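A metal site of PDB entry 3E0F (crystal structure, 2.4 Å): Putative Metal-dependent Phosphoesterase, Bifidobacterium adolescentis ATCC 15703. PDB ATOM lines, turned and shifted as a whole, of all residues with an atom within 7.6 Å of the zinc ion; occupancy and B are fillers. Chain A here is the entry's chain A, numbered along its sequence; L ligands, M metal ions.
The backbone NH (N) of His 20 is in hydrogen-bond range of the backbone carbonyl oxygen (O) of Trp 262, at 2.8 Å.
ND1 of His 263 sits close to NZ of Lys 267.
A ring nitrogen (ND1) of His 263 sits at hydrogen-bond distance from the backbone carbonyl oxygen (O) of Asp 261 (2.6 Å).
The backbone carbonyl oxygen of Asp 25 is in hydrogen-bond range of the guanidinium group of Arg 162.
OD1 of Asp 25 lies within hydrogen-bond range of OG of Ser 24, 3.5 Å away.
The backbone NH (N) of His 50 sits at hydrogen-bond distance from the side-chain hydroxyl (OG) of Ser 24 (3.3 Å).
The backbone carbonyl oxygen of Ala 48 lies close to a ring nitrogen (ND1) of His 20 (3.2 Å).
Merely in contact with the zinc ion: His 20.
Within 4 Å of the zinc ion: His 20, Asp 25, His 50 and His 263.
The zinc ion is bound by a ring nitrogen (NE2) of His 50 (2.1 Å), the side-chain carboxylate (OD2) of Asp 25 (2.1 Å), an oxygen (O3) of the ligand (2.3 Å) and a ring nitrogen (NE2) of His 263 (2.3 Å).
The zinc ion has four donor atoms within binding distance.
Slightly farther from the zinc ion lies O4 of the ligand (2.7 Å).
Slightly farther from the zinc ion lies OD1 of Asp 25 (2.8 Å).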
ATOM      1  N   HIS A  18      17.252   7.568   4.344  1.00  0.00           N
ATOM      2  CA  HIS A  18      16.036   6.763   4.480  1.00  0.00           C
ATOM      3  C   HIS A  18      15.895   5.719   3.319  1.00  0.00           C
ATOM      4  O   HIS A  18      15.186   5.906   2.334  1.00  0.00           O
ATOM      5  CB  HIS A  18      14.847   7.745   4.539  1.00  0.00           C
ATOM      6  CG  HIS A  18      13.566   7.135   4.987  1.00  0.00           C
ATOM      7  ND1 HIS A  18      12.468   7.902   5.332  1.00  0.00           N
ATOM      8  CD2 HIS A  18      13.187   5.840   5.142  1.00  0.00           C
ATOM      9  CE1 HIS A  18      11.478   7.096   5.673  1.00  0.00           C
ATOM     10  NE2 HIS A  18      11.875   5.851   5.556  1.00  0.00           N
ATOM     11  N   HIS A  20      15.667   1.375   2.363  1.00  0.00           N
ATOM     12  CA  HIS A  20      15.353   0.030   2.784  1.00  0.00           C
ATOM     13  C   HIS A  20      16.034  -1.029   1.896  1.00  0.00           C
ATOM     14  O   HIS A  20      16.221  -0.821   0.686  1.00  0.00           O
ATOM     15  CB  HIS A  20      13.850  -0.134   2.735  1.00  0.00           C
ATOM     16  CG  HIS A  20      13.131   0.802   3.651  1.00  0.00           C
ATOM     17  ND1 HIS A  20      12.832   0.478   4.949  1.00  0.00           N
ATOM     18  CD2 HIS A  20      12.697   2.071   3.476  1.00  0.00           C
ATOM     19  CE1 HIS A  20      12.232   1.497   5.534  1.00  0.00           C
ATOM     20  NE2 HIS A  20      12.128   2.470   4.654  1.00  0.00           N
ATOM     21  N   SER A  24      14.417  -5.754   5.346  1.00  0.00           N
ATOM     22  CA  SER A  24      13.021  -5.451   5.618  1.00  0.00           C
ATOM     23  C   SER A  24      12.274  -5.584   4.294  1.00  0.00           C
ATOM     24  O   SER A  24      12.168  -6.691   3.763  1.00  0.00           O
ATOM     25  CB  SER A  24      12.813  -4.102   6.345  1.00  0.00           C
ATOM     26  OG  SER A  24      13.335  -2.975   5.637  1.00  0.00           O
ATOM     27  N   ASP A  25      11.794  -4.492   3.704  1.00  0.00           N
ATOM     28  CA  ASP A  25      10.920  -4.568   2.530  1.00  0.00           C
ATOM     29  C   ASP A  25      11.459  -3.916   1.272  1.00  0.00           C
ATOM     30  O   ASP A  25      10.708  -3.674   0.339  1.00  0.00           O
ATOM     31  CB  ASP A  25       9.553  -3.971   2.845  1.00  0.00           C
ATOM     32  CG  ASP A  25       9.634  -2.523   3.345  1.00  0.00           C
ATOM     33  OD1 ASP A  25      10.753  -2.000   3.519  1.00  0.00           O
ATOM     34  OD2 ASP A  25       8.564  -1.926   3.589  1.00  0.00           O
ATOM     35  N   GLY A  26      12.758  -3.647   1.245  1.00  0.00           N
ATOM     36  CA  GLY A  26      13.424  -3.226   0.010  1.00  0.00           C
ATOM     37  C   GLY A  26      13.786  -4.437  -0.823  1.00  0.00           C
ATOM     38  O   GLY A  26      13.676  -5.554  -0.369  1.00  0.00           O
ATOM     39  N   ALA A  48      17.924   2.077   6.790  1.00  0.00           N
ATOM     40  CA  ALA A  48      16.767   2.448   7.652  1.00  0.00           C
ATOM     41  C   ALA A  48      15.667   1.377   7.600  1.00  0.00           C
ATOM     42  O   ALA A  48      14.487   1.680   7.366  1.00  0.00           O
ATOM     43  CB  ALA A  48      16.215   3.841   7.266  1.00  0.00           C
ATOM     44  N   ASP A  49      16.060   0.139   7.844  1.00  0.00           N
ATOM     45  CA  ASP A  49      15.142  -0.983   7.708  1.00  0.00           C
ATOM     46  C   ASP A  49      14.189  -0.998   8.875  1.00  0.00           C
ATOM     47  O   ASP A  49      14.535  -0.567   9.946  1.00  0.00           O
ATOM     48  CB  ASP A  49      15.893  -2.339   7.577  1.00  0.00           C
ATOM     49  CG  ASP A  49      16.516  -2.547   6.180  1.00  0.00           C
ATOM     50  OD1 ASP A  49      15.821  -2.327   5.167  1.00  0.00           O
ATOM     51  OD2 ASP A  49      17.704  -2.937   6.104  1.00  0.00           O
ATOM     52  N   HIS A  50      12.978  -1.503   8.624  1.00  0.00           N
ATOM     53  CA  HIS A  50      11.965  -1.643   9.648  1.00  0.00           C
ATOM     54  C   HIS A  50      12.372  -2.535  10.781  1.00  0.00           C
ATOM     55  O   HIS A  50      12.665  -3.711  10.562  1.00  0.00           O
ATOM     56  CB  HIS A  50      10.664  -2.193   9.083  1.00  0.00           C
ATOM     57  CG  HIS A  50      10.066  -1.345   8.030  1.00  0.00           C
ATOM     58  ND1 HIS A  50       9.453  -0.143   8.311  1.00  0.00           N
ATOM     59  CD2 HIS A  50      10.020  -1.488   6.688  1.00  0.00           C
ATOM     60  CE1 HIS A  50       9.011   0.395   7.189  1.00  0.00           C
ATOM     61  NE2 HIS A  50       9.342  -0.399   6.189  1.00  0.00           N
ATOM     62  N   GLU A  75      14.000   2.211  10.846  1.00  0.00           N
ATOM     63  CA  GLU A  75      12.695   2.835  10.877  1.00  0.00           C
ATOM     64  C   GLU A  75      11.793   2.022  11.817  1.00  0.00           C
ATOM     65  O   GLU A  75      11.627   0.822  11.672  1.00  0.00           O
ATOM     66  CB  GLU A  75      12.069   2.899   9.475  1.00  0.00           C
ATOM     67  CG  GLU A  75      10.723   3.595   9.476  1.00  0.00           C
ATOM     68  CD  GLU A  75      10.175   3.917   8.112  1.00  0.00           C
ATOM     69  OE1 GLU A  75      10.754   3.494   7.105  1.00  0.00           O
ATOM     70  OE2 GLU A  75       9.113   4.595   8.046  1.00  0.00           O
ATOM     71  N   HIS A  86       5.983   6.903  11.866  1.00  0.00           N
ATOM     72  CA  HIS A  86       7.214   6.169  11.624  1.00  0.00           C
ATOM     73  C   HIS A  86       8.390   7.028  12.082  1.00  0.00           C
ATOM     74  O   HIS A  86       8.417   8.244  11.842  1.00  0.00           O
ATOM     75  CB  HIS A  86       7.363   5.809  10.157  1.00  0.00           C
ATOM     76  CG  HIS A  86       6.321   4.873   9.637  1.00  0.00           C
ATOM     77  ND1 HIS A  86       6.430   4.239   8.411  1.00  0.00           N
ATOM     78  CD2 HIS A  86       5.166   4.423  10.178  1.00  0.00           C
ATOM     79  CE1 HIS A  86       5.374   3.476   8.217  1.00  0.00           C
ATOM     80  NE2 HIS A  86       4.593   3.568   9.276  1.00  0.00           N
ATOM     81  N   PRO A 147       4.391  -5.605   2.749  1.00  0.00           N
ATOM     82  CA  PRO A 147       4.990  -5.566   1.412  1.00  0.00           C
ATOM     83  C   PRO A 147       5.347  -6.928   0.827  1.00  0.00           C
ATOM     84  O   PRO A 147       5.352  -7.088  -0.397  1.00  0.00           O
ATOM     85  CB  PRO A 147       6.253  -4.737   1.608  1.00  0.00           C
ATOM     86  CG  PRO A 147       6.001  -3.959   2.846  1.00  0.00           C
ATOM     87  CD  PRO A 147       5.236  -4.866   3.714  1.00  0.00           C
ATOM     88  N   ARG A 162       3.318  -3.543  -6.406  1.00  0.00           N
ATOM     89  CA  ARG A 162       3.094  -3.573  -4.978  1.00  0.00           C
ATOM     90  C   ARG A 162       2.167  -2.420  -4.557  1.00  0.00           C
ATOM     91  O   ARG A 162       1.404  -2.540  -3.594  1.00  0.00           O
ATOM     92  CB  ARG A 162       4.452  -3.411  -4.302  1.00  0.00           C
ATOM     93  CG  ARG A 162       4.507  -3.826  -2.861  1.00  0.00           C
ATOM     94  CD  ARG A 162       5.760  -3.305  -2.174  1.00  0.00           C
ATOM     95  NE  ARG A 162       6.921  -4.196  -2.327  1.00  0.00           N
ATOM     96  CZ  ARG A 162       8.069  -4.006  -1.668  1.00  0.00           C
ATOM     97  NH1 ARG A 162       8.244  -2.942  -0.900  1.00  0.00           N
ATOM     98  NH2 ARG A 162       9.069  -4.875  -1.814  1.00  0.00           N
ATOM     99  N   PHE A 166      -1.402  -2.577  -2.362  1.00  0.00           N
ATOM    100  CA  PHE A 166      -1.706  -1.659  -1.246  1.00  0.00           C
ATOM    101  C   PHE A 166      -2.928  -0.755  -1.468  1.00  0.00           C
ATOM    102  O   PHE A 166      -3.478  -0.220  -0.513  1.00  0.00           O
ATOM    103  CB  PHE A 166      -0.519  -0.699  -0.976  1.00  0.00           C
ATOM    104  CG  PHE A 166       0.702  -1.344  -0.388  1.00  0.00           C
ATOM    105  CD1 PHE A 166       0.607  -2.342   0.560  1.00  0.00           C
ATOM    106  CD2 PHE A 166       1.964  -0.905  -0.746  1.00  0.00           C
ATOM    107  CE1 PHE A 166       1.747  -2.921   1.094  1.00  0.00           C
ATOM    108  CE2 PHE A 166       3.089  -1.477  -0.208  1.00  0.00           C
ATOM    109  CZ  PHE A 166       2.984  -2.486   0.715  1.00  0.00           C
ATOM    110  N   ASP A 261      13.211   7.160   0.861  1.00  0.00           N
ATOM    111  CA  ASP A 261      12.325   6.064   1.234  1.00  0.00           C
ATOM    112  C   ASP A 261      12.374   4.945   0.177  1.00  0.00           C
ATOM    113  O   ASP A 261      11.406   4.255  -0.101  1.00  0.00           O
ATOM    114  CB  ASP A 261      10.911   6.568   1.452  1.00  0.00           C
ATOM    115  CG  ASP A 261      10.251   5.895   2.555  1.00  0.00           C
ATOM    116  OD1 ASP A 261      10.670   4.782   2.857  1.00  0.00           O
ATOM    117  OD2 ASP A 261       9.333   6.471   3.140  1.00  0.00           O
ATOM    118  N   TRP A 262      13.550   4.819  -0.404  1.00  0.00           N
ATOM    119  CA  TRP A 262      13.826   3.881  -1.442  1.00  0.00           C
ATOM    120  C   TRP A 262      13.585   2.495  -0.934  1.00  0.00           C
ATOM    121  O   TRP A 262      14.061   2.127   0.142  1.00  0.00           O
ATOM    122  CB  TRP A 262      15.291   3.995  -1.775  1.00  0.00           C
ATOM    123  CG  TRP A 262      15.813   3.162  -2.877  1.00  0.00           C
ATOM    124  CD1 TRP A 262      15.544   3.296  -4.216  1.00  0.00           C
ATOM    125  CD2 TRP A 262      16.806   2.135  -2.763  1.00  0.00           C
ATOM    126  NE1 TRP A 262      16.290   2.388  -4.924  1.00  0.00           N
ATOM    127  CE2 TRP A 262      17.081   1.679  -4.060  1.00  0.00           C
ATOM    128  CE3 TRP A 262      17.486   1.566  -1.684  1.00  0.00           C
ATOM    129  CZ2 TRP A 262      17.988   0.675  -4.307  1.00  0.00           C
ATOM    130  CZ3 TRP A 262      18.384   0.582  -1.928  1.00  0.00           C
ATOM    131  CH2 TRP A 262      18.630   0.131  -3.223  1.00  0.00           C
ATOM    132  N   HIS A 263      12.868   1.721  -1.747  1.00  0.00           N
ATOM    133  CA  HIS A 263      12.700   0.320  -1.508  1.00  0.00           C
ATOM    134  C   HIS A 263      13.176  -0.438  -2.723  1.00  0.00           C
ATOM    135  O   HIS A 263      12.744  -1.554  -2.953  1.00  0.00           O
ATOM    136  CB  HIS A 263      11.228   0.003  -1.257  1.00  0.00           C
ATOM    137  CG  HIS A 263      10.731   0.483   0.062  1.00  0.00           C
ATOM    138  ND1 HIS A 263      10.648   1.813   0.392  1.00  0.00           N
ATOM    139  CD2 HIS A 263      10.271  -0.197   1.127  1.00  0.00           C
ATOM    140  CE1 HIS A 263      10.161   1.931   1.600  1.00  0.00           C
ATOM    141  NE2 HIS A 263       9.923   0.728   2.069  1.00  0.00           N
ATOM    142  N   LYS A 267       9.072   0.165  -4.874  1.00  0.00           N
ATOM    143  CA  LYS A 267       8.436   1.483  -4.873  1.00  0.00           C
ATOM    144  C   LYS A 267       8.984   2.305  -6.036  1.00  0.00           C
ATOM    145  O   LYS A 267      10.102   2.063  -6.492  1.00  0.00           O
ATOM    146  CB  LYS A 267       8.760   2.263  -3.582  1.00  0.00           C
ATOM    147  CG  LYS A 267       8.135   1.738  -2.287  1.00  0.00           C
ATOM    148  CD  LYS A 267       7.091   2.652  -1.723  1.00  0.00           C
ATOM    149  CE  LYS A 267       7.047   2.621  -0.178  1.00  0.00           C
ATOM    150  NZ  LYS A 267       7.967   3.651   0.474  1.00  0.00           N
HETATM  151  P1  LIG L   1       7.692   2.673   4.521  1.00  0.00           P
HETATM  152  O1  LIG L   1       7.352   3.622   3.377  1.00  0.00           O
HETATM  153  O2  LIG L   1       7.194   3.105   5.893  1.00  0.00           O
HETATM  154  O3  LIG L   1       7.129   1.316   4.152  1.00  0.00           O
HETATM  155  O4  LIG L   1       9.198   2.679   4.703  1.00  0.00           O
HETATM  156 ZN    ZN M   1       9.056   0.092   4.127  1.00  0.00          ZN
HETATM  157 FE    FE M   2      10.578   4.113   5.125  1.00  0.00          FE
HETATM  158 FE    FE M   3       7.602   4.891   6.707  1.00  0.00          FE
